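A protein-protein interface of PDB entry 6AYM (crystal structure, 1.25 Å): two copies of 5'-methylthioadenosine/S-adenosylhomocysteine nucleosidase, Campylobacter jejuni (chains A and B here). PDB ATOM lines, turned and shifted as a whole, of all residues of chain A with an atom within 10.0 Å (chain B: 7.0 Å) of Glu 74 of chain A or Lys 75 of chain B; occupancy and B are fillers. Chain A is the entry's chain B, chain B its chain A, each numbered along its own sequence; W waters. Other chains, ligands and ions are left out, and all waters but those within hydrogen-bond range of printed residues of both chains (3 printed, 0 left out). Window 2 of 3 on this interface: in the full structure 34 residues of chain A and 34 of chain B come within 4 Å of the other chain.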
ATOM      1  N   LYS A  12     -21.524  13.678 -17.791  1.00  0.00           N
ATOM      2  CA  LYS A  12     -21.477  14.035 -19.203  1.00  0.00           C
ATOM      3  C   LYS A  12     -22.881  14.362 -19.697  1.00  0.00           C
ATOM      4  O   LYS A  12     -23.815  13.588 -19.470  1.00  0.00           O
ATOM      5  CB  LYS A  12     -20.903  12.892 -20.023  1.00  0.00           C
ATOM      6  CG  LYS A  12     -20.578  13.341 -21.415  1.00  0.00           C
ATOM      7  CD  LYS A  12     -19.883  12.231 -22.179  1.00  0.00           C
ATOM      8  CE  LYS A  12     -19.178  12.827 -23.391  1.00  0.00           C
ATOM      9  NZ  LYS A  12     -18.183  11.886 -23.926  1.00  0.00           N
ATOM     10  N   ALA A  14     -25.529  15.485 -22.778  1.00  0.00           N
ATOM     11  CA  ALA A  14     -25.895  15.670 -24.184  1.00  0.00           C
ATOM     12  C   ALA A  14     -26.840  16.846 -24.329  1.00  0.00           C
ATOM     13  O   ALA A  14     -27.795  16.967 -23.563  1.00  0.00           O
ATOM     14  CB  ALA A  14     -26.546  14.417 -24.739  1.00  0.00           C
ATOM     15  N   HIS A  38     -20.413  11.415 -37.936  1.00  0.00           N
ATOM     16  CA  HIS A  38     -20.806  10.078 -37.521  1.00  0.00           C
ATOM     17  C   HIS A  38     -22.298   9.966 -37.693  1.00  0.00           C
ATOM     18  O   HIS A  38     -23.017  10.923 -37.460  1.00  0.00           O
ATOM     19  CB  HIS A  38     -20.426   9.805 -36.062  1.00  0.00           C
ATOM     20  CG  HIS A  38     -20.708   8.399 -35.616  1.00  0.00           C
ATOM     21  ND1 HIS A  38     -19.965   7.325 -36.053  1.00  0.00           N
ATOM     22  CD2 HIS A  38     -21.675   7.883 -34.806  1.00  0.00           C
ATOM     23  CE1 HIS A  38     -20.434   6.217 -35.513  1.00  0.00           C
ATOM     24  NE2 HIS A  38     -21.486   6.524 -34.773  1.00  0.00           N
ATOM     25  N   TYR A  43     -21.409  15.534 -34.572  1.00  0.00           N
ATOM     26  CA  TYR A  43     -21.468  15.584 -33.113  1.00  0.00           C
ATOM     27  C   TYR A  43     -20.312  16.435 -32.625  1.00  0.00           C
ATOM     28  O   TYR A  43     -19.180  16.269 -33.075  1.00  0.00           O
ATOM     29  CB  TYR A  43     -21.436  14.170 -32.538  1.00  0.00           C
ATOM     30  CG  TYR A  43     -22.678  13.399 -32.917  1.00  0.00           C
ATOM     31  CD1 TYR A  43     -23.750  13.336 -32.053  1.00  0.00           C
ATOM     32  CD2 TYR A  43     -22.776  12.733 -34.145  1.00  0.00           C
ATOM     33  CE1 TYR A  43     -24.925  12.682 -32.407  1.00  0.00           C
ATOM     34  CE2 TYR A  43     -23.945  12.096 -34.529  1.00  0.00           C
ATOM     35  CZ  TYR A  43     -25.000  12.045 -33.633  1.00  0.00           C
ATOM     36  OH  TYR A  43     -26.151  11.391 -33.975  1.00  0.00           O
ATOM     37  N   VAL A  54     -21.670  16.832 -25.148  1.00  0.00           N
ATOM     38  CA  VAL A  54     -21.775  16.380 -26.529  1.00  0.00           C
ATOM     39  C   VAL A  54     -23.019  17.057 -27.092  1.00  0.00           C
ATOM     40  O   VAL A  54     -24.069  17.030 -26.444  1.00  0.00           O
ATOM     41  CB  VAL A  54     -21.803  14.841 -26.687  1.00  0.00           C
ATOM     42  CG1 VAL A  54     -22.863  14.159 -25.833  1.00  0.00           C
ATOM     43  CG2 VAL A  54     -21.945  14.466 -28.147  1.00  0.00           C
ATOM     44  N   THR A  66     -34.368   9.676 -32.834  1.00  0.00           N
ATOM     45  CA  THR A  66     -34.090   8.444 -32.098  1.00  0.00           C
ATOM     46  C   THR A  66     -32.632   8.042 -32.291  1.00  0.00           C
ATOM     47  O   THR A  66     -31.936   7.717 -31.319  1.00  0.00           O
ATOM     48  CB  THR A  66     -34.993   7.293 -32.578  1.00  0.00           C
ATOM     49  OG1 THR A  66     -36.363   7.640 -32.332  1.00  0.00           O
ATOM     50  CG2 THR A  66     -34.679   5.975 -31.857  1.00  0.00           C
ATOM     51  N   LEU A  67     -32.186   8.056 -33.544  1.00  0.00           N
ATOM     52  CA  LEU A  67     -30.799   7.713 -33.835  1.00  0.00           C
ATOM     53  C   LEU A  67     -29.819   8.668 -33.144  1.00  0.00           C
ATOM     54  O   LEU A  67     -28.868   8.221 -32.499  1.00  0.00           O
ATOM     55  CB  LEU A  67     -30.568   7.694 -35.349  1.00  0.00           C
ATOM     56  CG  LEU A  67     -29.134   7.451 -35.829  1.00  0.00           C
ATOM     57  CD1 LEU A  67     -28.560   6.153 -35.280  1.00  0.00           C
ATOM     58  CD2 LEU A  67     -29.138   7.436 -37.344  1.00  0.00           C
ATOM     59  N   SER A  68     -30.064   9.969 -33.240  1.00  0.00           N
ATOM     60  CA  SER A  68     -29.149  10.932 -32.627  1.00  0.00           C
ATOM     61  C   SER A  68     -29.037  10.743 -31.110  1.00  0.00           C
ATOM     62  O   SER A  68     -27.955  10.729 -30.548  1.00  0.00           O
ATOM     63  CB  SER A  68     -29.591  12.350 -32.955  1.00  0.00           C
ATOM     64  OG  SER A  68     -29.485  12.641 -34.347  1.00  0.00           O
ATOM     65  N   ALA A  69     -30.168  10.577 -30.443  1.00  0.00           N
ATOM     66  CA  ALA A  69     -30.147  10.342 -28.998  1.00  0.00           C
ATOM     67  C   ALA A  69     -29.437   9.036 -28.640  1.00  0.00           C
ATOM     68  O   ALA A  69     -28.657   9.001 -27.670  1.00  0.00           O
ATOM     69  CB  ALA A  69     -31.554  10.359 -28.438  1.00  0.00           C
ATOM     70  N   SER A  70     -29.683   7.978 -29.414  1.00  0.00           N
ATOM     71  CA  SER A  70     -29.055   6.692 -29.148  1.00  0.00           C
ATOM     72  C   SER A  70     -27.539   6.769 -29.320  1.00  0.00           C
ATOM     73  O   SER A  70     -26.799   6.183 -28.531  1.00  0.00           O
ATOM     74  CB  SER A  70     -29.629   5.607 -30.039  1.00  0.00           C
ATOM     75  OG  SER A  70     -28.980   4.385 -29.765  1.00  0.00           O
ATOM     76  N   VAL A  71     -27.077   7.514 -30.330  1.00  0.00           N
ATOM     77  CA  VAL A  71     -25.639   7.734 -30.539  1.00  0.00           C
ATOM     78  C   VAL A  71     -25.048   8.498 -29.362  1.00  0.00           C
ATOM     79  O   VAL A  71     -23.990   8.113 -28.819  1.00  0.00           O
ATOM     80  CB  VAL A  71     -25.398   8.469 -31.870  1.00  0.00           C
ATOM     81  CG1 VAL A  71     -23.965   9.018 -31.976  1.00  0.00           C
ATOM     82  CG2 VAL A  71     -25.693   7.535 -33.039  1.00  0.00           C
ATOM     83  N   MET A  72     -25.710   9.559 -28.935  1.00  0.00           N
ATOM     84  CA  MET A  72     -25.189  10.365 -27.841  1.00  0.00           C
ATOM     85  C   MET A  72     -24.993   9.564 -26.555  1.00  0.00           C
ATOM     86  O   MET A  72     -24.034   9.779 -25.812  1.00  0.00           O
ATOM     87  CB  MET A  72     -26.066  11.581 -27.613  1.00  0.00           C
ATOM     88  CG  MET A  72     -26.008  12.538 -28.781  1.00  0.00           C
ATOM     89  SD  MET A  72     -27.179  13.889 -28.707  1.00  0.00           S
ATOM     90  CE  MET A  72     -26.032  15.262 -28.489  1.00  0.00           C
ATOM     91  N   ILE A  73     -25.891   8.616 -26.308  1.00  0.00           N
ATOM     92  CA  ILE A  73     -25.819   7.809 -25.100  1.00  0.00           C
ATOM     93  C   ILE A  73     -24.971   6.565 -25.321  1.00  0.00           C
ATOM     94  O   ILE A  73     -24.013   6.346 -24.557  1.00  0.00           O
ATOM     95  CB  ILE A  73     -27.228   7.425 -24.635  1.00  0.00           C
ATOM     96  CG1 ILE A  73     -28.021   8.688 -24.256  1.00  0.00           C
ATOM     97  CG2 ILE A  73     -27.132   6.472 -23.441  1.00  0.00           C
ATOM     98  CD1 ILE A  73     -29.519   8.486 -24.151  1.00  0.00           C
ATOM     99  N   GLU A  74     -25.297   5.746 -26.321  1.00  0.00           N
ATOM    100  CA  GLU A  74     -24.612   4.456 -26.491  1.00  0.00           C
ATOM    101  C   GLU A  74     -23.181   4.595 -26.992  1.00  0.00           C
ATOM    102  O   GLU A  74     -22.331   3.793 -26.589  1.00  0.00           O
ATOM    103  CB  GLU A  74     -25.379   3.510 -27.429  1.00  0.00           C
ATOM    104  CG  GLU A  74     -26.781   3.150 -26.974  1.00  0.00           C
ATOM    105  CD  GLU A  74     -26.817   2.322 -25.695  1.00  0.00           C
ATOM    106  OE1 GLU A  74     -27.217   1.136 -25.768  1.00  0.00           O
ATOM    107  OE2 GLU A  74     -26.480   2.865 -24.618  1.00  0.00           O
ATOM    108  N   LYS A  75     -22.912   5.565 -27.863  1.00  0.00           N
ATOM    109  CA  LYS A  75     -21.537   5.793 -28.329  1.00  0.00           C
ATOM    110  C   LYS A  75     -20.804   6.795 -27.449  1.00  0.00           C
ATOM    111  O   LYS A  75     -19.706   6.492 -26.955  1.00  0.00           O
ATOM    112  CB  LYS A  75     -21.510   6.242 -29.785  1.00  0.00           C
ATOM    113  CG  LYS A  75     -20.101   6.411 -30.348  1.00  0.00           C
ATOM    114  CD  LYS A  75     -20.121   6.708 -31.818  1.00  0.00           C
ATOM    115  CE  LYS A  75     -18.735   7.038 -32.368  1.00  0.00           C
ATOM    116  NZ  LYS A  75     -17.810   5.894 -32.273  1.00  0.00           N
ATOM    117  N   PHE A  76     -21.392   7.961 -27.206  1.00  0.00           N
ATOM    118  CA  PHE A  76     -20.668   9.033 -26.533  1.00  0.00           C
ATOM    119  C   PHE A  76     -20.879   9.127 -25.023  1.00  0.00           C
ATOM    120  O   PHE A  76     -20.309  10.006 -24.405  1.00  0.00           O
ATOM    121  CB  PHE A  76     -20.917  10.363 -27.248  1.00  0.00           C
ATOM    122  CG  PHE A  76     -20.477  10.369 -28.688  1.00  0.00           C
ATOM    123  CD1 PHE A  76     -19.167  10.026 -29.022  1.00  0.00           C
ATOM    124  CD2 PHE A  76     -21.367  10.698 -29.709  1.00  0.00           C
ATOM    125  CE1 PHE A  76     -18.765  10.010 -30.344  1.00  0.00           C
ATOM    126  CE2 PHE A  76     -20.968  10.706 -31.021  1.00  0.00           C
ATOM    127  CZ  PHE A  76     -19.671  10.340 -31.345  1.00  0.00           C
ATOM    128  N   GLY A  77     -21.654   8.216 -24.428  1.00  0.00           N
ATOM    129  CA  GLY A  77     -21.725   8.091 -22.985  1.00  0.00           C
ATOM    130  C   GLY A  77     -22.427   9.210 -22.255  1.00  0.00           C
ATOM    131  O   GLY A  77     -22.165   9.448 -21.071  1.00  0.00           O
ATOM    132  N   ALA A  78     -23.356   9.903 -22.926  1.00  0.00           N
ATOM    133  CA  ALA A  78     -24.104  10.947 -22.245  1.00  0.00           C
ATOM    134  C   ALA A  78     -24.909  10.343 -21.091  1.00  0.00           C
ATOM    135  O   ALA A  78     -25.486   9.262 -21.228  1.00  0.00           O
ATOM    136  CB  ALA A  78     -25.026  11.636 -23.219  1.00  0.00           C
ATOM    137  N   GLN A  79     -24.915  11.063 -19.964  1.00  0.00           N
ATOM    138  CA  GLN A  79     -25.573  10.625 -18.730  1.00  0.00           C
ATOM    139  C   GLN A  79     -26.849  11.409 -18.428  1.00  0.00           C
ATOM    140  O   GLN A  79     -27.670  10.960 -17.627  1.00  0.00           O
ATOM    141  CB  GLN A  79     -24.583  10.740 -17.577  1.00  0.00           C
ATOM    142  CG  GLN A  79     -23.423   9.768 -17.689  1.00  0.00           C
ATOM    143  CD  GLN A  79     -22.299  10.071 -16.715  1.00  0.00           C
ATOM    144  OE1 GLN A  79     -21.651  11.109 -16.795  1.00  0.00           O
ATOM    145  NE2 GLN A  79     -22.050   9.144 -15.801  1.00  0.00           N
ATOM    146  N   LEU A  81     -29.610  14.135 -20.861  1.00  0.00           N
ATOM    147  CA  LEU A  81     -29.875  14.715 -22.176  1.00  0.00           C
ATOM    148  C   LEU A  81     -30.881  15.856 -22.067  1.00  0.00           C
ATOM    149  O   LEU A  81     -31.981  15.675 -21.540  1.00  0.00           O
ATOM    150  CB  LEU A  81     -30.325  13.629 -23.155  1.00  0.00           C
ATOM    151  CG  LEU A  81     -30.416  14.071 -24.626  1.00  0.00           C
ATOM    152  CD1 LEU A  81     -30.082  12.912 -25.569  1.00  0.00           C
ATOM    153  CD2 LEU A  81     -31.796  14.645 -24.938  1.00  0.00           C
ATOM    154  N   VAL A 190     -36.058   6.961 -25.956  1.00  0.00           N
ATOM    155  CA  VAL A 190     -34.682   6.480 -25.952  1.00  0.00           C
ATOM    156  C   VAL A 190     -34.027   6.691 -24.591  1.00  0.00           C
ATOM    157  O   VAL A 190     -33.421   5.771 -24.015  1.00  0.00           O
ATOM    158  CB  VAL A 190     -33.841   7.175 -27.039  1.00  0.00           C
ATOM    159  CG1 VAL A 190     -32.358   6.852 -26.891  1.00  0.00           C
ATOM    160  CG2 VAL A 190     -34.306   6.783 -28.423  1.00  0.00           C
ATOM    161  N   CYS A 191     -34.185   7.903 -24.054  1.00  0.00           N
ATOM    162  CA  CYS A 191     -33.560   8.245 -22.778  1.00  0.00           C
ATOM    163  C   CYS A 191     -34.088   7.391 -21.646  1.00  0.00           C
ATOM    164  O   CYS A 191     -33.310   6.839 -20.874  1.00  0.00           O
ATOM    165  CB  CYS A 191     -33.750   9.725 -22.468  1.00  0.00           C
ATOM    166  SG  CYS A 191     -32.788  10.799 -23.548  1.00  0.00           S
ATOM    167  N   ALA A 193     -35.440   4.413 -21.901  1.00  0.00           N
ATOM    168  CA  ALA A 193     -35.007   3.030 -22.114  1.00  0.00           C
ATOM    169  C   ALA A 193     -33.563   2.821 -21.653  1.00  0.00           C
ATOM    170  O   ALA A 193     -33.210   1.748 -21.147  1.00  0.00           O
ATOM    171  CB  ALA A 193     -35.156   2.657 -23.569  1.00  0.00           C
ATOM    172  N   LEU A 194     -32.730   3.838 -21.832  1.00  0.00           N
ATOM    173  CA  LEU A 194     -31.317   3.768 -21.487  1.00  0.00           C
ATOM    174  C   LEU A 194     -30.999   4.359 -20.104  1.00  0.00           C
ATOM    175  O   LEU A 194     -29.834   4.509 -19.753  1.00  0.00           O
ATOM    176  CB  LEU A 194     -30.498   4.452 -22.583  1.00  0.00           C
ATOM    177  CG  LEU A 194     -30.600   3.767 -23.954  1.00  0.00           C
ATOM    178  CD1 LEU A 194     -29.905   4.593 -25.008  1.00  0.00           C
ATOM    179  CD2 LEU A 194     -30.030   2.358 -23.933  1.00  0.00           C
ATOM    180  N   LYS A 195     -32.028   4.651 -19.321  1.00  0.00           N
ATOM    181  CA  LYS A 195     -31.884   5.144 -17.939  1.00  0.00           C
ATOM    182  C   LYS A 195     -31.106   6.455 -17.849  1.00  0.00           C
ATOM    183  O   LYS A 195     -30.282   6.658 -16.952  1.00  0.00           O
ATOM    184  CB  LYS A 195     -31.288   4.067 -17.025  1.00  0.00           C
ATOM    185  CG  LYS A 195     -32.103   2.775 -17.055  1.00  0.00           C
ATOM    186  CD  LYS A 195     -31.591   1.734 -16.074  1.00  0.00           C
ATOM    187  CE  LYS A 195     -32.042   0.347 -16.486  1.00  0.00           C
ATOM    188  NZ  LYS A 195     -33.516   0.266 -16.699  1.00  0.00           N
ATOM    189  N   VAL A 196     -31.392   7.342 -18.795  1.00  0.00           N
ATOM    190  CA  VAL A 196     -30.766   8.658 -18.876  1.00  0.00           C
ATOM    191  C   VAL A 196     -31.853   9.709 -18.637  1.00  0.00           C
ATOM    192  O   VAL A 196     -32.833   9.759 -19.370  1.00  0.00           O
ATOM    193  CB  VAL A 196     -30.116   8.857 -20.265  1.00  0.00           C
ATOM    194  CG1 VAL A 196     -29.713  10.304 -20.529  1.00  0.00           C
ATOM    195  CG2 VAL A 196     -28.910   7.947 -20.400  1.00  0.00           C
ATOM    196  N   LYS B  12     -18.876  -9.632 -36.902  1.00  0.00           N
ATOM    197  CA  LYS B  12     -19.988  -9.732 -35.969  1.00  0.00           C
ATOM    198  C   LYS B  12     -21.294  -9.388 -36.687  1.00  0.00           C
ATOM    199  O   LYS B  12     -21.391  -8.347 -37.334  1.00  0.00           O
ATOM    200  CB  LYS B  12     -19.798  -8.811 -34.777  1.00  0.00           C
ATOM    201  CG  LYS B  12     -20.830  -9.106 -33.698  1.00  0.00           C
ATOM    202  CD  LYS B  12     -20.679  -8.306 -32.447  1.00  0.00           C
ATOM    203  CE  LYS B  12     -19.578  -8.771 -31.531  1.00  0.00           C
ATOM    204  NZ  LYS B  12     -19.747  -8.064 -30.230  1.00  0.00           N
ATOM    205  N   HIS B  38     -31.369  -4.919 -21.970  1.00  0.00           N
ATOM    206  CA  HIS B  38     -30.780  -3.599 -22.205  1.00  0.00           C
ATOM    207  C   HIS B  38     -31.748  -2.788 -23.039  1.00  0.00           C
ATOM    208  O   HIS B  38     -32.427  -3.348 -23.891  1.00  0.00           O
ATOM    209  CB  HIS B  38     -29.442  -3.744 -22.920  1.00  0.00           C
ATOM    210  CG  HIS B  38     -28.716  -2.448 -23.133  1.00  0.00           C
ATOM    211  ND1 HIS B  38     -28.122  -1.742 -22.112  1.00  0.00           N
ATOM    212  CD2 HIS B  38     -28.513  -1.720 -24.256  1.00  0.00           C
ATOM    213  CE1 HIS B  38     -27.550  -0.655 -22.606  1.00  0.00           C
ATOM    214  NE2 HIS B  38     -27.784  -0.611 -23.907  1.00  0.00           N
ATOM    215  N   ALA B  39     -31.843  -1.490 -22.771  1.00  0.00           N
ATOM    216  CA  ALA B  39     -32.665  -0.598 -23.601  1.00  0.00           C
ATOM    217  C   ALA B  39     -34.129  -1.086 -23.667  1.00  0.00           C
ATOM    218  O   ALA B  39     -34.773  -1.026 -24.706  1.00  0.00           O
ATOM    219  CB  ALA B  39     -32.066  -0.453 -24.993  1.00  0.00           C
ATOM    220  N   LEU B  67     -34.077   2.289 -32.477  1.00  0.00           N
ATOM    221  CA  LEU B  67     -33.332   2.110 -31.240  1.00  0.00           C
ATOM    222  C   LEU B  67     -32.650   0.734 -31.211  1.00  0.00           C
ATOM    223  O   LEU B  67     -31.469   0.641 -30.919  1.00  0.00           O
ATOM    224  CB  LEU B  67     -34.256   2.288 -30.022  1.00  0.00           C
ATOM    225  CG  LEU B  67     -33.621   2.040 -28.656  1.00  0.00           C
ATOM    226  CD1 LEU B  67     -32.396   2.910 -28.421  1.00  0.00           C
ATOM    227  CD2 LEU B  67     -34.637   2.242 -27.552  1.00  0.00           C
ATOM    228  N   ALA B  69     -31.741  -1.344 -33.665  1.00  0.00           N
ATOM    229  CA  ALA B  69     -30.615  -1.388 -34.589  1.00  0.00           C
ATOM    230  C   ALA B  69     -29.422  -0.557 -34.116  1.00  0.00           C
ATOM    231  O   ALA B  69     -28.276  -1.007 -34.213  1.00  0.00           O
ATOM    232  CB  ALA B  69     -31.053  -0.957 -35.972  1.00  0.00           C
ATOM    233  N   SER B  70     -29.693   0.635 -33.579  1.00  0.00           N
ATOM    234  CA  SER B  70     -28.624   1.514 -33.094  1.00  0.00           C
ATOM    235  C   SER B  70     -27.879   0.865 -31.924  1.00  0.00           C
ATOM    236  O   SER B  70     -26.654   0.959 -31.827  1.00  0.00           O
ATOM    237  CB  SER B  70     -29.181   2.867 -32.639  1.00  0.00           C
ATOM    238  OG  SER B  70     -29.817   3.591 -33.672  1.00  0.00           O
ATOM    239  N   VAL B  71     -28.610   0.201 -31.037  1.00  0.00           N
ATOM    240  CA  VAL B  71     -27.998  -0.523 -29.907  1.00  0.00           C
ATOM    241  C   VAL B  71     -27.140  -1.672 -30.420  1.00  0.00           C
ATOM    242  O   VAL B  71     -25.995  -1.845 -29.986  1.00  0.00           O
ATOM    243  CB  VAL B  71     -29.095  -1.046 -28.954  1.00  0.00           C
ATOM    244  CG1 VAL B  71     -28.556  -2.058 -27.968  1.00  0.00           C
ATOM    245  CG2 VAL B  71     -29.714   0.115 -28.205  1.00  0.00           C
ATOM    246  N   MET B  72     -27.644  -2.444 -31.367  1.00  0.00           N
ATOM    247  CA  MET B  72     -26.890  -3.585 -31.879  1.00  0.00           C
ATOM    248  C   MET B  72     -25.554  -3.162 -32.480  1.00  0.00           C
ATOM    249  O   MET B  72     -24.545  -3.865 -32.324  1.00  0.00           O
ATOM    250  CB  MET B  72     -27.708  -4.372 -32.880  1.00  0.00           C
ATOM    251  CG  MET B  72     -28.883  -5.049 -32.222  1.00  0.00           C
ATOM    252  SD  MET B  72     -30.016  -5.820 -33.387  1.00  0.00           S
ATOM    253  CE  MET B  72     -29.671  -7.548 -33.090  1.00  0.00           C
ATOM    254  N   ILE B  73     -25.534  -2.002 -33.128  1.00  0.00           N
ATOM    255  CA  ILE B  73     -24.323  -1.504 -33.763  1.00  0.00           C
ATOM    256  C   ILE B  73     -23.479  -0.701 -32.794  1.00  0.00           C
ATOM    257  O   ILE B  73     -22.305  -1.021 -32.599  1.00  0.00           O
ATOM    258  CB  ILE B  73     -24.687  -0.673 -35.005  1.00  0.00           C
ATOM    259  CG1 ILE B  73     -25.393  -1.554 -36.047  1.00  0.00           C
ATOM    260  CG2 ILE B  73     -23.450  -0.016 -35.592  1.00  0.00           C
ATOM    261  CD1 ILE B  73     -26.146  -0.799 -37.128  1.00  0.00           C
ATOM    262  N   GLU B  74     -24.040   0.336 -32.181  1.00  0.00           N
ATOM    263  CA  GLU B  74     -23.231   1.254 -31.347  1.00  0.00           C
ATOM    264  C   GLU B  74     -22.809   0.636 -30.016  1.00  0.00           C
ATOM    265  O   GLU B  74     -21.705   0.891 -29.544  1.00  0.00           O
ATOM    266  CB  GLU B  74     -23.953   2.578 -31.081  1.00  0.00           C
ATOM    267  CG  GLU B  74     -24.354   3.379 -32.317  1.00  0.00           C
ATOM    268  CD  GLU B  74     -23.196   3.911 -33.118  1.00  0.00           C
ATOM    269  OE1 GLU B  74     -23.063   5.130 -33.196  1.00  0.00           O
ATOM    270  OE2 GLU B  74     -22.449   3.114 -33.715  1.00  0.00           O
ATOM    271  N   LYS B  75     -23.675  -0.160 -29.401  1.00  0.00           N
ATOM    272  CA  LYS B  75     -23.354  -0.805 -28.129  1.00  0.00           C
ATOM    273  C   LYS B  75     -22.702  -2.164 -28.325  1.00  0.00           C
ATOM    274  O   LYS B  75     -21.673  -2.437 -27.715  1.00  0.00           O
ATOM    275  CB  LYS B  75     -24.607  -0.914 -27.250  1.00  0.00           C
ATOM    276  CG  LYS B  75     -24.350  -1.466 -25.856  1.00  0.00           C
ATOM    277  CD  LYS B  75     -23.316  -0.686 -25.034  1.00  0.00           C
ATOM    278  CE  LYS B  75     -23.601   0.807 -24.913  1.00  0.00           C
ATOM    279  NZ  LYS B  75     -22.503   1.551 -24.221  1.00  0.00           N
ATOM    280  N   PHE B  76     -23.285  -3.017 -29.163  1.00  0.00           N
ATOM    281  CA  PHE B  76     -22.817  -4.401 -29.289  1.00  0.00           C
ATOM    282  C   PHE B  76     -21.914  -4.672 -30.493  1.00  0.00           C
ATOM    283  O   PHE B  76     -21.514  -5.818 -30.693  1.00  0.00           O
ATOM    284  CB  PHE B  76     -24.011  -5.363 -29.210  1.00  0.00           C
ATOM    285  CG  PHE B  76     -24.782  -5.248 -27.908  1.00  0.00           C
ATOM    286  CD1 PHE B  76     -24.130  -5.389 -26.680  1.00  0.00           C
ATOM    287  CD2 PHE B  76     -26.152  -5.021 -27.912  1.00  0.00           C
ATOM    288  CE1 PHE B  76     -24.816  -5.260 -25.500  1.00  0.00           C
ATOM    289  CE2 PHE B  76     -26.833  -4.901 -26.715  1.00  0.00           C
ATOM    290  CZ  PHE B  76     -26.177  -5.038 -25.518  1.00  0.00           C
ATOM    291  N   GLY B  77     -21.569  -3.654 -31.276  1.00  0.00           N
ATOM    292  CA  GLY B  77     -20.528  -3.789 -32.294  1.00  0.00           C
ATOM    293  C   GLY B  77     -20.874  -4.580 -33.533  1.00  0.00           C
ATOM    294  O   GLY B  77     -19.988  -5.071 -34.225  1.00  0.00           O
ATOM    295  N   ALA B  78     -22.153  -4.730 -33.848  1.00  0.00           N
ATOM    296  CA  ALA B  78     -22.533  -5.440 -35.076  1.00  0.00           C
ATOM    297  C   ALA B  78     -21.968  -4.748 -36.308  1.00  0.00           C
ATOM    298  O   ALA B  78     -21.987  -3.530 -36.396  1.00  0.00           O
ATOM    299  CB  ALA B  78     -24.044  -5.539 -35.189  1.00  0.00           C
HETATM  300  O   HOH W   1     -30.894   0.073 -20.582  1.00  0.00           O
HETATM  301  O   HOH W   2     -22.629   4.260 -23.232  1.00  0.00           O
HETATM  302  O   HOH W   3     -20.382   1.545 -26.608  1.00  0.00           O
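The side-chain amino group of Lys 75 of chain B is in hydrogen-bond range of the backbone carbonyl oxygen of Glu 74 of chain A, at 3.3 Å.
OE1 of Glu 74 of chain B sits at hydrogen-bond distance from NE2 of His 38 of chain A.
A ring nitrogen (NE2) of His 38 of chain B sits at hydrogen-bond distance from the side-chain carboxylate (OE1) of Glu 74 of chain A, at 2.6 Å.
CG2 of Thr 66 of chain A touches N of Leu 67 of chain B, at 3.8 Å.
Ser 70 of chain B touches Leu 67 of chain A.
CD1 of Leu 67 of chain B touches OG of Ser 70 of chain A, at 3.96 Å.
Ser 70 of chain B touches Ser 70 of chain A (CB to OG, 3.3 Å).
Glu 74 of chain B touches Val 71 of chain A (OE1 to CG2, 3.6 Å).
Glu 74 of chain A touches Val 71 of chain B.
CD of Lys 75 of chain A touches OE1 of Glu 74 of chain B (3.6 Å).
CA of Ala 39 of chain B touches O of Ala 193 of chain A, at 3.4 Å.
His 38 of chain B touches Leu 194 of chain A (NE2 to CD2, 3.7 Å).
CB of Ala 39 of chain B touches CD2 of Leu 194 of chain A, 3.6 Å away.
Glu 74 of chain A touches three residues of chain B.
Of chain A, only Glu 74 comes within 4 Å of Lys 75 of chain B.
Of chain A, only Glu 74 (3.6 Å) comes within 4 Å of Val 71 of chain B.
Of the printed residues of chain B, Val 71 of chain A touches Glu 74.
Printed residues of chain A within 4 Å of Glu 74 of chain B: His 38, Val 71 and Lys 75.
The nearest residue of chain A that does not touch Lys 75 of chain B is Ile 73 of chain A (5.0 Å).
The backbone carbonyl oxygen of Val 71 of chain A sits at hydrogen-bond distance from the backbone NH of Phe 76 of chain A (3.1 Å).
The backbone NH (N) of Phe 76 of chain B lies within hydrogen-bond range of the backbone carbonyl oxygen (O) of Val 71 of chain B, at 3.1 Å.
Printed residues of chain B that touch a printed residue of chain A: His 38, Ala 39, Leu 67, Ser 70, Val 71, Glu 74 and Lys 75.
Hydrophobic or aromatic side chains of chain B that line the printed part of chain A: His 38, Ala 39, Leu 67 and Val 71.
Of the 26 printed residues of chain A, 9 touch a printed residue of chain B.
Printed residues of chain A that touch a printed residue of chain B: His 38, Thr 66, Leu 67, Ser 70, Val 71, Glu 74, Lys 75, Ala 193 and Leu 194.
Along chain A the printed residues that touch a printed residue of chain B span positions 38 to 194.
Among the printed residues, no Asp or Glu carboxylate lies within 4 Å of a Lys or Arg side-chain nitrogen of the other chain.
Leu 67 of chain A touches Ser 70 of chain B, and with the chains exchanged Ser 70 of chain A touches Leu 67 of chain B.
Ser 70 of chain B touches its own counterpart, Ser 70 of chain A.
Val 71 of chain A touches Glu 74 of chain B, and with the chains exchanged Glu 74 of chain A touches Val 71 of chain B.
Glu 74 of chain A touches Lys 75 of chain B, and with the chains exchanged Lys 75 of chain A touches Glu 74 of chain B.
Positions printed for both chains: 12, 38, 67, 69, 70, 71, 72, 73, 74, 75, 76, 77 and 78.
Water W2 lies within hydrogen-bond range of the backbone carbonyl oxygen (O) of Ile 73 of chain A (2.8 Å), the side-chain amino group (NZ) of Lys 75 of chain B (2.9 Å) and the backbone carbonyl oxygen (O) of Glu 74 of chain A (3.4 Å).
Water W1 bridges the backbone NH of Ala 39 of chain B and the backbone carbonyl oxygen of Ala 193 of chain A.
Water W3 lies within hydrogen-bond range of O of Glu 74 of chain A (3.0 Å), NZ of Lys 75 of chain B (3.2 Å) and O of Glu 74 of chain B (3.3 Å).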
